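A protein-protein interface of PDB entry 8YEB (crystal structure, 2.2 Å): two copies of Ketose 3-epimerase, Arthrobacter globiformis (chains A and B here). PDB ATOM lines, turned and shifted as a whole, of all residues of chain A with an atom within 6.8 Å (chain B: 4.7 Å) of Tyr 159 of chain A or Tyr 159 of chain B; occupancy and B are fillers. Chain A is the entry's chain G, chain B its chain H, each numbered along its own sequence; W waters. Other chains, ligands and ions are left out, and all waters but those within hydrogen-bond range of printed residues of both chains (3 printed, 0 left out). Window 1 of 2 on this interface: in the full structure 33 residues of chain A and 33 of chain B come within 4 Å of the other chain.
Asn 157 of chain A touches Tyr 159 of chain B, and with the chains exchanged Tyr 159 of chain A touches Asn 157 of chain B.
Of the 20 pairs that touch across the chains among the printed residues, 14 have their exchanged pair printed and touching as well.
Of the 11 printed residues of chain B, 9 touch a printed residue of chain A.
Printed residues of chain B that touch a printed residue of chain A: Lys 120, Asn 157, Arg 158, Tyr 159, Glu 160, Thr 161, Tyr 189, Arg 219 and Leu 263.
Hydrophobic or aromatic side chains of chain B within 4 Å of the printed part of chain A: Tyr 159 and Tyr 189.
Of the 21 printed residues of chain A, 11 touch a printed residue of chain B.
Along chain A the printed residues that touch a printed residue of chain B span positions 120 to 266.
Among the printed residues, no Asp or Glu carboxylate lies within 4 Å of a Lys or Arg side-chain nitrogen of the other chain.
ND2 of Asn 165 of chain A lies close to N of Arg 158 of chain A (3.5 Å).
The guanidinium group (NE) of Arg 158 of chain A is in salt-bridge range of the side-chain carboxylate (OE2) of Glu 194 of chain A (2.9 Å).
Water W2 lies within hydrogen-bond range of NZ of Lys 120 of chain B (2.5 Å) and O of Met 262 of chain A (3.1 Å).
The indole nitrogen (NE1) of Trp 266 of chain A is in hydrogen-bond range of the backbone carbonyl oxygen (O) of Arg 158 of chain B, 2.8 Å away.
OH of Tyr 159 of chain A sits at hydrogen-bond distance from OE2 of Glu 160 of chain B (2.4 Å).
NE1 of Trp 266 of chain A is in hydrogen-bond range of O of Thr 161 of chain B, 3.3 Å away.
OH of Tyr 159 of chain A sits at hydrogen-bond distance from OH of Tyr 189 of chain B, 2.7 Å away.
The backbone carbonyl oxygen (O) of Met 262 of chain A lies within hydrogen-bond range of the side-chain amino group (NZ) of Lys 120 of chain B, 3.2 Å away.
ND2 of Asn 157 of chain A is in hydrogen-bond range of OH of Tyr 159 of chain B, at 3.2 Å.
The side-chain hydroxyl (OH) of Tyr 159 of chain A is in hydrogen-bond range of the side-chain amide nitrogen (ND2) of Asn 157 of chain B (3.3 Å).
The side-chain hydroxyl (OH) of Tyr 189 of chain A lies within hydrogen-bond range of the side-chain hydroxyl (OH) of Tyr 159 of chain B.
The side-chain carboxylate of Glu 160 of chain A lies close to the side-chain hydroxyl of Tyr 159 of chain B.
Among the printed residues, merely in contact across the chains: Tyr 159 of chain A with Tyr 159 of chain B (3.3 Å), Gly 264 of chain A with Arg 158 of chain B (3.5 Å), Arg 158 of chain A with Tyr 189 of chain B (3.6 Å), Arg 219 of chain A with Arg 158 of chain B (3.6 Å), Arg 158 of chain A with Arg 219 of chain B (3.7 Å), Tyr 189 of chain A with Arg 158 of chain B (3.7 Å), Lys 120 of chain A with Lys 120 of chain B (3.7 Å), Leu 263 of chain A with Arg 158 of chain B (3.7 Å), Gly 264 of chain A with Lys 120 of chain B (3.8 Å), Arg 158 of chain A with Leu 263 of chain B (3.8 Å) and Leu 263 of chain A with Tyr 159 of chain B (3.9 Å).
Printed residues of chain B within 4 Å of Arg 158 of chain A: Tyr 189, Arg 219 and Leu 263.
Ile 193 of chain A touches none of the printed residues of chain B.
Of chain A, only Asn 157, Tyr 159, Glu 160, Tyr 189 and Leu 263 come within 4 Å of Tyr 159 of chain B.
Of the printed residues of chain A, Thr 161 of chain B touches Trp 266.
His 190 of chain B touches none of the printed residues of chain A.
The nearest residue of chain A that does not touch Tyr 159 of chain B is Arg 219 of chain A (4.3 Å).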
ATOM      1  N   MET A 118     -29.360 -22.661  11.515  1.00  0.00           N
ATOM      2  CA  MET A 118     -28.692 -21.573  12.209  1.00  0.00           C
ATOM      3  C   MET A 118     -28.967 -21.782  13.689  1.00  0.00           C
ATOM      4  O   MET A 118     -30.009 -21.377  14.211  1.00  0.00           O
ATOM      5  CB  MET A 118     -29.180 -20.192  11.741  1.00  0.00           C
ATOM      6  CG  MET A 118     -28.466 -19.015  12.403  1.00  0.00           C
ATOM      7  SD  MET A 118     -28.914 -17.423  11.605  1.00  0.00           S
ATOM      8  CE  MET A 118     -30.521 -17.166  12.346  1.00  0.00           C
ATOM      9  N   LYS A 119     -28.058 -22.515  14.327  1.00  0.00           N
ATOM     10  CA  LYS A 119     -28.280 -22.933  15.691  1.00  0.00           C
ATOM     11  C   LYS A 119     -26.999 -23.491  16.271  1.00  0.00           C
ATOM     12  O   LYS A 119     -26.026 -23.668  15.543  1.00  0.00           O
ATOM     13  CB  LYS A 119     -29.349 -24.025  15.749  1.00  0.00           C
ATOM     14  CG  LYS A 119     -28.958 -25.326  15.071  1.00  0.00           C
ATOM     15  CD  LYS A 119     -29.783 -26.466  15.598  1.00  0.00           C
ATOM     16  CE  LYS A 119     -29.359 -27.801  15.053  1.00  0.00           C
ATOM     17  NZ  LYS A 119     -30.090 -28.892  15.738  1.00  0.00           N
ATOM     18  N   LYS A 120     -27.049 -23.789  17.569  1.00  0.00           N
ATOM     19  CA  LYS A 120     -26.005 -24.534  18.256  1.00  0.00           C
ATOM     20  C   LYS A 120     -26.255 -26.034  18.095  1.00  0.00           C
ATOM     21  O   LYS A 120     -26.966 -26.630  18.904  1.00  0.00           O
ATOM     22  CB  LYS A 120     -25.981 -24.187  19.751  1.00  0.00           C
ATOM     23  CG  LYS A 120     -24.976 -24.953  20.606  1.00  0.00           C
ATOM     24  CD  LYS A 120     -23.548 -24.853  20.093  1.00  0.00           C
ATOM     25  CE  LYS A 120     -22.536 -25.796  20.716  1.00  0.00           C
ATOM     26  NZ  LYS A 120     -23.093 -26.930  21.499  1.00  0.00           N
ATOM     27  N   TYR A 121     -25.618 -26.625  17.083  1.00  0.00           N
ATOM     28  CA  TYR A 121     -25.533 -28.067  16.932  1.00  0.00           C
ATOM     29  C   TYR A 121     -24.900 -28.704  18.166  1.00  0.00           C
ATOM     30  O   TYR A 121     -24.087 -28.077  18.842  1.00  0.00           O
ATOM     31  CB  TYR A 121     -24.719 -28.448  15.691  1.00  0.00           C
ATOM     32  CG  TYR A 121     -25.464 -28.258  14.394  1.00  0.00           C
ATOM     33  CD1 TYR A 121     -25.638 -26.996  13.848  1.00  0.00           C
ATOM     34  CD2 TYR A 121     -26.075 -29.333  13.759  1.00  0.00           C
ATOM     35  CE1 TYR A 121     -26.322 -26.820  12.658  1.00  0.00           C
ATOM     36  CE2 TYR A 121     -26.796 -29.169  12.588  1.00  0.00           C
ATOM     37  CZ  TYR A 121     -26.933 -27.900  12.044  1.00  0.00           C
ATOM     38  OH  TYR A 121     -27.614 -27.701  10.879  1.00  0.00           O
ATOM     39  N   VAL A 156     -20.336 -18.235   9.723  1.00  0.00           N
ATOM     40  CA  VAL A 156     -20.811 -17.855  11.050  1.00  0.00           C
ATOM     41  C   VAL A 156     -20.101 -18.707  12.102  1.00  0.00           C
ATOM     42  O   VAL A 156     -19.477 -19.725  11.807  1.00  0.00           O
ATOM     43  CB  VAL A 156     -22.345 -17.910  11.208  1.00  0.00           C
ATOM     44  CG1 VAL A 156     -23.072 -16.960  10.272  1.00  0.00           C
ATOM     45  CG2 VAL A 156     -22.905 -19.319  11.063  1.00  0.00           C
ATOM     46  N   ASN A 157     -20.134 -18.236  13.339  1.00  0.00           N
ATOM     47  CA  ASN A 157     -19.372 -18.874  14.388  1.00  0.00           C
ATOM     48  C   ASN A 157     -19.945 -20.250  14.766  1.00  0.00           C
ATOM     49  O   ASN A 157     -21.098 -20.591  14.453  1.00  0.00           O
ATOM     50  CB  ASN A 157     -19.284 -17.947  15.599  1.00  0.00           C
ATOM     51  CG  ASN A 157     -20.581 -17.808  16.344  1.00  0.00           C
ATOM     52  OD1 ASN A 157     -21.068 -18.768  16.936  1.00  0.00           O
ATOM     53  ND2 ASN A 157     -21.126 -16.606  16.345  1.00  0.00           N
ATOM     54  N   ARG A 158     -19.144 -20.969  15.554  1.00  0.00           N
ATOM     55  CA  ARG A 158     -19.389 -22.347  15.981  1.00  0.00           C
ATOM     56  C   ARG A 158     -20.710 -22.579  16.728  1.00  0.00           C
ATOM     57  O   ARG A 158     -21.138 -23.725  16.836  1.00  0.00           O
ATOM     58  CB  ARG A 158     -18.263 -22.801  16.913  1.00  0.00           C
ATOM     59  CG  ARG A 158     -18.228 -22.011  18.217  1.00  0.00           C
ATOM     60  CD  ARG A 158     -16.932 -22.108  19.000  1.00  0.00           C
ATOM     61  NE  ARG A 158     -15.753 -21.871  18.172  1.00  0.00           N
ATOM     62  CZ  ARG A 158     -14.509 -22.139  18.536  1.00  0.00           C
ATOM     63  NH1 ARG A 158     -14.265 -22.764  19.678  1.00  0.00           N
ATOM     64  NH2 ARG A 158     -13.515 -21.813  17.730  1.00  0.00           N
ATOM     65  N   TYR A 159     -21.347 -21.533  17.254  1.00  0.00           N
ATOM     66  CA  TYR A 159     -22.585 -21.667  18.004  1.00  0.00           C
ATOM     67  C   TYR A 159     -23.805 -21.439  17.110  1.00  0.00           C
ATOM     68  O   TYR A 159     -24.947 -21.485  17.574  1.00  0.00           O
ATOM     69  CB  TYR A 159     -22.635 -20.631  19.121  1.00  0.00           C
ATOM     70  CG  TYR A 159     -21.516 -20.698  20.122  1.00  0.00           C
ATOM     71  CD1 TYR A 159     -21.491 -21.679  21.106  1.00  0.00           C
ATOM     72  CD2 TYR A 159     -20.493 -19.765  20.107  1.00  0.00           C
ATOM     73  CE1 TYR A 159     -20.494 -21.703  22.066  1.00  0.00           C
ATOM     74  CE2 TYR A 159     -19.494 -19.775  21.057  1.00  0.00           C
ATOM     75  CZ  TYR A 159     -19.488 -20.756  22.031  1.00  0.00           C
ATOM     76  OH  TYR A 159     -18.474 -20.749  22.944  1.00  0.00           O
ATOM     77  N   GLU A 160     -23.565 -21.163  15.828  1.00  0.00           N
ATOM     78  CA  GLU A 160     -24.636 -20.894  14.886  1.00  0.00           C
ATOM     79  C   GLU A 160     -24.555 -21.827  13.667  1.00  0.00           C
ATOM     80  O   GLU A 160     -25.507 -21.888  12.888  1.00  0.00           O
ATOM     81  CB  GLU A 160     -24.591 -19.424  14.477  1.00  0.00           C
ATOM     82  CG  GLU A 160     -24.996 -18.472  15.589  1.00  0.00           C
ATOM     83  CD  GLU A 160     -25.203 -17.027  15.155  1.00  0.00           C
ATOM     84  OE1 GLU A 160     -25.581 -16.812  14.009  1.00  0.00           O
ATOM     85  OE2 GLU A 160     -24.916 -16.107  15.949  1.00  0.00           O
ATOM     86  N   THR A 161     -23.420 -22.524  13.465  1.00  0.00           N
ATOM     87  CA  THR A 161     -23.342 -23.638  12.517  1.00  0.00           C
ATOM     88  C   THR A 161     -22.174 -24.549  12.882  1.00  0.00           C
ATOM     89  O   THR A 161     -21.232 -24.117  13.565  1.00  0.00           O
ATOM     90  CB  THR A 161     -23.100 -23.191  11.067  1.00  0.00           C
ATOM     91  OG1 THR A 161     -23.275 -24.306  10.185  1.00  0.00           O
ATOM     92  CG2 THR A 161     -21.712 -22.610  10.850  1.00  0.00           C
ATOM     93  N   ASN A 162     -22.215 -25.774  12.338  1.00  0.00           N
ATOM     94  CA  ASN A 162     -21.098 -26.699  12.433  1.00  0.00           C
ATOM     95  C   ASN A 162     -20.467 -26.972  11.065  1.00  0.00           C
ATOM     96  O   ASN A 162     -19.615 -27.840  10.943  1.00  0.00           O
ATOM     97  CB  ASN A 162     -21.495 -28.019  13.100  1.00  0.00           C
ATOM     98  CG  ASN A 162     -22.593 -28.781  12.388  1.00  0.00           C
ATOM     99  OD1 ASN A 162     -23.049 -28.395  11.318  1.00  0.00           O
ATOM    100  ND2 ASN A 162     -23.046 -29.851  13.010  1.00  0.00           N
ATOM    101  N   ASN A 165     -17.391 -22.298   9.394  1.00  0.00           N
ATOM    102  CA  ASN A 165     -17.018 -21.411  10.493  1.00  0.00           C
ATOM    103  C   ASN A 165     -15.875 -20.464  10.121  1.00  0.00           C
ATOM    104  O   ASN A 165     -15.628 -19.505  10.852  1.00  0.00           O
ATOM    105  CB  ASN A 165     -16.604 -22.166  11.762  1.00  0.00           C
ATOM    106  CG  ASN A 165     -17.716 -22.995  12.385  1.00  0.00           C
ATOM    107  OD1 ASN A 165     -17.483 -24.103  12.842  1.00  0.00           O
ATOM    108  ND2 ASN A 165     -18.923 -22.485  12.447  1.00  0.00           N
ATOM    109  N   TYR A 189     -18.473  -9.733  12.917  1.00  0.00           N
ATOM    110  CA  TYR A 189     -18.836 -10.275  14.219  1.00  0.00           C
ATOM    111  C   TYR A 189     -18.393 -11.724  14.319  1.00  0.00           C
ATOM    112  O   TYR A 189     -17.847 -12.129  15.332  1.00  0.00           O
ATOM    113  CB  TYR A 189     -20.347 -10.170  14.457  1.00  0.00           C
ATOM    114  CG  TYR A 189     -20.887 -11.013  15.580  1.00  0.00           C
ATOM    115  CD1 TYR A 189     -20.675 -10.686  16.914  1.00  0.00           C
ATOM    116  CD2 TYR A 189     -21.604 -12.161  15.304  1.00  0.00           C
ATOM    117  CE1 TYR A 189     -21.205 -11.455  17.936  1.00  0.00           C
ATOM    118  CE2 TYR A 189     -22.134 -12.940  16.315  1.00  0.00           C
ATOM    119  CZ  TYR A 189     -21.931 -12.595  17.635  1.00  0.00           C
ATOM    120  OH  TYR A 189     -22.480 -13.416  18.598  1.00  0.00           O
ATOM    121  N   HIS A 190     -18.663 -12.495  13.263  1.00  0.00           N
ATOM    122  CA  HIS A 190     -18.303 -13.912  13.228  1.00  0.00           C
ATOM    123  C   HIS A 190     -16.793 -14.091  13.042  1.00  0.00           C
ATOM    124  O   HIS A 190     -16.183 -14.962  13.659  1.00  0.00           O
ATOM    125  CB  HIS A 190     -19.135 -14.632  12.162  1.00  0.00           C
ATOM    126  CG  HIS A 190     -20.604 -14.642  12.483  1.00  0.00           C
ATOM    127  ND1 HIS A 190     -21.110 -15.259  13.616  1.00  0.00           N
ATOM    128  CD2 HIS A 190     -21.661 -14.101  11.847  1.00  0.00           C
ATOM    129  CE1 HIS A 190     -22.418 -15.117  13.632  1.00  0.00           C
ATOM    130  NE2 HIS A 190     -22.781 -14.412  12.582  1.00  0.00           N
ATOM    131  N   ILE A 193     -14.467 -14.084  16.102  1.00  0.00           N
ATOM    132  CA  ILE A 193     -14.351 -15.300  16.892  1.00  0.00           C
ATOM    133  C   ILE A 193     -13.440 -16.299  16.185  1.00  0.00           C
ATOM    134  O   ILE A 193     -12.431 -16.683  16.751  1.00  0.00           O
ATOM    135  CB  ILE A 193     -15.749 -15.874  17.220  1.00  0.00           C
ATOM    136  CG1 ILE A 193     -16.551 -14.858  18.051  1.00  0.00           C
ATOM    137  CG2 ILE A 193     -15.618 -17.234  17.908  1.00  0.00           C
ATOM    138  CD1 ILE A 193     -18.053 -15.052  18.022  1.00  0.00           C
ATOM    139  N   GLU A 194     -13.740 -16.642  14.937  1.00  0.00           N
ATOM    140  CA  GLU A 194     -13.202 -17.848  14.331  1.00  0.00           C
ATOM    141  C   GLU A 194     -11.882 -17.628  13.586  1.00  0.00           C
ATOM    142  O   GLU A 194     -11.046 -18.552  13.568  1.00  0.00           O
ATOM    143  CB  GLU A 194     -14.247 -18.486  13.410  1.00  0.00           C
ATOM    144  CG  GLU A 194     -15.550 -18.865  14.124  1.00  0.00           C
ATOM    145  CD  GLU A 194     -15.435 -19.981  15.151  1.00  0.00           C
ATOM    146  OE1 GLU A 194     -14.384 -20.650  15.166  1.00  0.00           O
ATOM    147  OE2 GLU A 194     -16.392 -20.145  15.983  1.00  0.00           O
ATOM    148  N   ARG A 219     -22.409  -6.949  18.856  1.00  0.00           N
ATOM    149  CA  ARG A 219     -23.480  -6.667  17.909  1.00  0.00           C
ATOM    150  C   ARG A 219     -24.194  -5.366  18.227  1.00  0.00           C
ATOM    151  O   ARG A 219     -25.261  -5.145  17.685  1.00  0.00           O
ATOM    152  CB  ARG A 219     -24.469  -7.822  17.825  1.00  0.00           C
ATOM    153  CG  ARG A 219     -23.798  -9.187  17.752  1.00  0.00           C
ATOM    154  CD  ARG A 219     -24.687 -10.263  17.164  1.00  0.00           C
ATOM    155  NE  ARG A 219     -24.610 -10.247  15.721  1.00  0.00           N
ATOM    156  CZ  ARG A 219     -24.898 -11.279  14.927  1.00  0.00           C
ATOM    157  NH1 ARG A 219     -24.533 -11.211  13.674  1.00  0.00           N
ATOM    158  NH2 ARG A 219     -25.441 -12.401  15.381  1.00  0.00           N
ATOM    159  N   MET A 262     -32.818 -17.258  18.505  1.00  0.00           N
ATOM    160  CA  MET A 262     -31.839 -18.081  17.804  1.00  0.00           C
ATOM    161  C   MET A 262     -30.435 -17.471  17.930  1.00  0.00           C
ATOM    162  O   MET A 262     -29.454 -18.200  18.021  1.00  0.00           O
ATOM    163  CB  MET A 262     -32.209 -18.212  16.322  1.00  0.00           C
ATOM    164  CG  MET A 262     -33.450 -19.102  16.031  1.00  0.00           C
ATOM    165  SD  MET A 262     -34.076 -18.880  14.323  1.00  0.00           S
ATOM    166  CE  MET A 262     -33.136 -20.104  13.401  1.00  0.00           C
ATOM    167  N   LEU A 263     -30.344 -16.133  17.960  1.00  0.00           N
ATOM    168  CA  LEU A 263     -29.067 -15.426  18.015  1.00  0.00           C
ATOM    169  C   LEU A 263     -28.660 -15.097  19.448  1.00  0.00           C
ATOM    170  O   LEU A 263     -27.580 -14.578  19.661  1.00  0.00           O
ATOM    171  CB  LEU A 263     -29.180 -14.129  17.204  1.00  0.00           C
ATOM    172  CG  LEU A 263     -29.489 -14.319  15.721  1.00  0.00           C
ATOM    173  CD1 LEU A 263     -29.358 -13.002  14.985  1.00  0.00           C
ATOM    174  CD2 LEU A 263     -28.555 -15.350  15.112  1.00  0.00           C
ATOM    175  N   GLY A 264     -29.527 -15.359  20.425  1.00  0.00           N
ATOM    176  CA  GLY A 264     -29.160 -15.206  21.819  1.00  0.00           C
ATOM    177  C   GLY A 264     -29.053 -13.740  22.207  1.00  0.00           C
ATOM    178  O   GLY A 264     -28.123 -13.360  22.908  1.00  0.00           O
ATOM    179  N   TRP A 266     -29.945 -11.394  24.483  1.00  0.00           N
ATOM    180  CA  TRP A 266     -30.465 -11.311  25.843  1.00  0.00           C
ATOM    181  C   TRP A 266     -30.428  -9.870  26.373  1.00  0.00           C
ATOM    182  O   TRP A 266     -31.156  -9.548  27.303  1.00  0.00           O
ATOM    183  CB  TRP A 266     -29.686 -12.244  26.802  1.00  0.00           C
ATOM    184  CG  TRP A 266     -29.321 -13.611  26.292  1.00  0.00           C
ATOM    185  CD1 TRP A 266     -28.100 -14.226  26.350  1.00  0.00           C
ATOM    186  CD2 TRP A 266     -30.207 -14.550  25.659  1.00  0.00           C
ATOM    187  NE1 TRP A 266     -28.160 -15.471  25.783  1.00  0.00           N
ATOM    188  CE2 TRP A 266     -29.446 -15.696  25.347  1.00  0.00           C
ATOM    189  CE3 TRP A 266     -31.571 -14.517  25.321  1.00  0.00           C
ATOM    190  CZ2 TRP A 266     -30.007 -16.802  24.709  1.00  0.00           C
ATOM    191  CZ3 TRP A 266     -32.124 -15.606  24.690  1.00  0.00           C
ATOM    192  CH2 TRP A 266     -31.357 -16.744  24.417  1.00  0.00           C
ATOM    193  N   LYS B 119     -25.032 -23.665  28.134  1.00  0.00           N
ATOM    194  CA  LYS B 119     -25.669 -24.060  26.897  1.00  0.00           C
ATOM    195  C   LYS B 119     -26.210 -22.844  26.176  1.00  0.00           C
ATOM    196  O   LYS B 119     -26.202 -21.737  26.703  1.00  0.00           O
ATOM    197  CB  LYS B 119     -26.855 -24.988  27.158  1.00  0.00           C
ATOM    198  CG  LYS B 119     -27.968 -24.386  28.007  1.00  0.00           C
ATOM    199  CD  LYS B 119     -29.268 -25.154  27.846  1.00  0.00           C
ATOM    200  CE  LYS B 119     -30.442 -24.489  28.520  1.00  0.00           C
ATOM    201  NZ  LYS B 119     -31.710 -25.156  28.153  1.00  0.00           N
ATOM    202  N   LYS B 120     -26.688 -23.097  24.967  1.00  0.00           N
ATOM    203  CA  LYS B 120     -27.418 -22.103  24.206  1.00  0.00           C
ATOM    204  C   LYS B 120     -28.874 -22.129  24.636  1.00  0.00           C
ATOM    205  O   LYS B 120     -29.628 -22.944  24.121  1.00  0.00           O
ATOM    206  CB  LYS B 120     -27.314 -22.393  22.700  1.00  0.00           C
ATOM    207  CG  LYS B 120     -28.118 -21.453  21.811  1.00  0.00           C
ATOM    208  CD  LYS B 120     -27.765 -19.991  22.017  1.00  0.00           C
ATOM    209  CE  LYS B 120     -28.800 -18.990  21.558  1.00  0.00           C
ATOM    210  NZ  LYS B 120     -29.974 -19.596  20.892  1.00  0.00           N
ATOM    211  N   ASN B 157     -20.130 -16.132  27.170  1.00  0.00           N
ATOM    212  CA  ASN B 157     -20.835 -15.467  26.089  1.00  0.00           C
ATOM    213  C   ASN B 157     -22.291 -15.934  26.027  1.00  0.00           C
ATOM    214  O   ASN B 157     -22.686 -16.905  26.688  1.00  0.00           O
ATOM    215  CB  ASN B 157     -20.114 -15.637  24.756  1.00  0.00           C
ATOM    216  CG  ASN B 157     -20.152 -17.041  24.214  1.00  0.00           C
ATOM    217  OD1 ASN B 157     -21.211 -17.512  23.796  1.00  0.00           O
ATOM    218  ND2 ASN B 157     -18.991 -17.687  24.152  1.00  0.00           N
ATOM    219  N   ARG B 158     -23.042 -15.222  25.176  1.00  0.00           N
ATOM    220  CA  ARG B 158     -24.481 -15.322  25.004  1.00  0.00           C
ATOM    221  C   ARG B 158     -24.918 -16.730  24.613  1.00  0.00           C
ATOM    222  O   ARG B 158     -26.057 -17.125  24.859  1.00  0.00           O
ATOM    223  CB  ARG B 158     -24.911 -14.305  23.936  1.00  0.00           C
ATOM    224  CG  ARG B 158     -24.264 -14.493  22.568  1.00  0.00           C
ATOM    225  CD  ARG B 158     -24.633 -13.381  21.595  1.00  0.00           C
ATOM    226  NE  ARG B 158     -24.076 -12.129  22.082  1.00  0.00           N
ATOM    227  CZ  ARG B 158     -24.455 -10.909  21.728  1.00  0.00           C
ATOM    228  NH1 ARG B 158     -25.247 -10.708  20.691  1.00  0.00           N
ATOM    229  NH2 ARG B 158     -24.016  -9.874  22.418  1.00  0.00           N
ATOM    230  N   TYR B 159     -24.030 -17.469  23.953  1.00  0.00           N
ATOM    231  CA  TYR B 159     -24.366 -18.791  23.472  1.00  0.00           C
ATOM    232  C   TYR B 159     -24.099 -19.866  24.525  1.00  0.00           C
ATOM    233  O   TYR B 159     -24.415 -21.018  24.246  1.00  0.00           O
ATOM    234  CB  TYR B 159     -23.578 -19.135  22.218  1.00  0.00           C
ATOM    235  CG  TYR B 159     -23.678 -18.167  21.068  1.00  0.00           C
ATOM    236  CD1 TYR B 159     -24.784 -18.140  20.230  1.00  0.00           C
ATOM    237  CD2 TYR B 159     -22.629 -17.311  20.787  1.00  0.00           C
ATOM    238  CE1 TYR B 159     -24.847 -17.268  19.152  1.00  0.00           C
ATOM    239  CE2 TYR B 159     -22.669 -16.446  19.711  1.00  0.00           C
ATOM    240  CZ  TYR B 159     -23.782 -16.415  18.892  1.00  0.00           C
ATOM    241  OH  TYR B 159     -23.760 -15.564  17.819  1.00  0.00           O
ATOM    242  N   GLU B 160     -23.536 -19.509  25.696  1.00  0.00           N
ATOM    243  CA  GLU B 160     -23.274 -20.479  26.759  1.00  0.00           C
ATOM    244  C   GLU B 160     -24.024 -20.153  28.066  1.00  0.00           C
ATOM    245  O   GLU B 160     -24.064 -20.973  28.991  1.00  0.00           O
ATOM    246  CB  GLU B 160     -21.772 -20.576  27.031  1.00  0.00           C
ATOM    247  CG  GLU B 160     -20.976 -21.060  25.851  1.00  0.00           C
ATOM    248  CD  GLU B 160     -19.550 -21.526  26.132  1.00  0.00           C
ATOM    249  OE1 GLU B 160     -19.152 -21.665  27.314  1.00  0.00           O
ATOM    250  OE2 GLU B 160     -18.819 -21.720  25.160  1.00  0.00           O
ATOM    251  N   THR B 161     -24.583 -18.946  28.184  1.00  0.00           N
ATOM    252  CA  THR B 161     -25.485 -18.618  29.280  1.00  0.00           C
ATOM    253  C   THR B 161     -26.360 -17.447  28.853  1.00  0.00           C
ATOM    254  O   THR B 161     -25.975 -16.670  27.979  1.00  0.00           O
ATOM    255  CB  THR B 161     -24.779 -18.223  30.586  1.00  0.00           C
ATOM    256  OG1 THR B 161     -25.738 -18.109  31.651  1.00  0.00           O
ATOM    257  CG2 THR B 161     -24.046 -16.900  30.469  1.00  0.00           C
ATOM    258  N   TYR B 189     -11.532 -15.215  25.997  1.00  0.00           N
ATOM    259  CA  TYR B 189     -12.348 -15.718  24.889  1.00  0.00           C
ATOM    260  C   TYR B 189     -13.769 -15.130  24.907  1.00  0.00           C
ATOM    261  O   TYR B 189     -14.285 -14.725  23.865  1.00  0.00           O
ATOM    262  CB  TYR B 189     -12.400 -17.248  24.953  1.00  0.00           C
ATOM    263  CG  TYR B 189     -13.437 -17.917  24.072  1.00  0.00           C
ATOM    264  CD1 TYR B 189     -13.281 -17.992  22.687  1.00  0.00           C
ATOM    265  CD2 TYR B 189     -14.579 -18.499  24.627  1.00  0.00           C
ATOM    266  CE1 TYR B 189     -14.233 -18.605  21.883  1.00  0.00           C
ATOM    267  CE2 TYR B 189     -15.532 -19.135  23.836  1.00  0.00           C
ATOM    268  CZ  TYR B 189     -15.360 -19.176  22.460  1.00  0.00           C
ATOM    269  OH  TYR B 189     -16.259 -19.796  21.651  1.00  0.00           O
ATOM    270  N   HIS B 190     -14.388 -15.097  26.095  1.00  0.00           N
ATOM    271  CA  HIS B 190     -15.752 -14.625  26.293  1.00  0.00           C
ATOM    272  C   HIS B 190     -15.785 -13.094  26.283  1.00  0.00           C
ATOM    273  O   HIS B 190     -16.705 -12.495  25.749  1.00  0.00           O
ATOM    274  CB  HIS B 190     -16.330 -15.231  27.581  1.00  0.00           C
ATOM    275  CG  HIS B 190     -16.464 -16.722  27.524  1.00  0.00           C
ATOM    276  ND1 HIS B 190     -17.289 -17.351  26.604  1.00  0.00           N
ATOM    277  CD2 HIS B 190     -15.880 -17.709  28.256  1.00  0.00           C
ATOM    278  CE1 HIS B 190     -17.208 -18.661  26.777  1.00  0.00           C
ATOM    279  NE2 HIS B 190     -16.362 -18.904  27.777  1.00  0.00           N
ATOM    280  N   ARG B 219      -9.986 -20.212  20.465  1.00  0.00           N
ATOM    281  CA  ARG B 219      -9.647 -21.193  21.499  1.00  0.00           C
ATOM    282  C   ARG B 219      -8.475 -22.079  21.059  1.00  0.00           C
ATOM    283  O   ARG B 219      -8.244 -23.124  21.654  1.00  0.00           O
ATOM    284  CB  ARG B 219     -10.855 -22.045  21.932  1.00  0.00           C
ATOM    285  CG  ARG B 219     -12.065 -21.217  22.333  1.00  0.00           C
ATOM    286  CD  ARG B 219     -13.197 -21.873  23.095  1.00  0.00           C
ATOM    287  NE  ARG B 219     -13.027 -21.676  24.525  1.00  0.00           N
ATOM    288  CZ  ARG B 219     -13.980 -21.787  25.443  1.00  0.00           C
ATOM    289  NH1 ARG B 219     -13.708 -21.417  26.675  1.00  0.00           N
ATOM    290  NH2 ARG B 219     -15.201 -22.200  25.137  1.00  0.00           N
ATOM    291  N   LEU B 263     -19.307 -27.203  23.794  1.00  0.00           N
ATOM    292  CA  LEU B 263     -18.496 -26.025  23.532  1.00  0.00           C
ATOM    293  C   LEU B 263     -18.384 -25.765  22.031  1.00  0.00           C
ATOM    294  O   LEU B 263     -17.865 -24.732  21.630  1.00  0.00           O
ATOM    295  CB  LEU B 263     -17.122 -26.211  24.193  1.00  0.00           C
ATOM    296  CG  LEU B 263     -17.134 -26.185  25.725  1.00  0.00           C
ATOM    297  CD1 LEU B 263     -15.740 -26.053  26.281  1.00  0.00           C
ATOM    298  CD2 LEU B 263     -17.980 -25.059  26.289  1.00  0.00           C
HETATM  299  O   HOH W   1     -16.066 -22.832  22.417  1.00  0.00           O
HETATM  300  O   HOH W   2     -29.849 -21.170  18.909  1.00  0.00           O
HETATM  301  O   HOH W   3     -25.717 -13.090  18.454  1.00  0.00           O
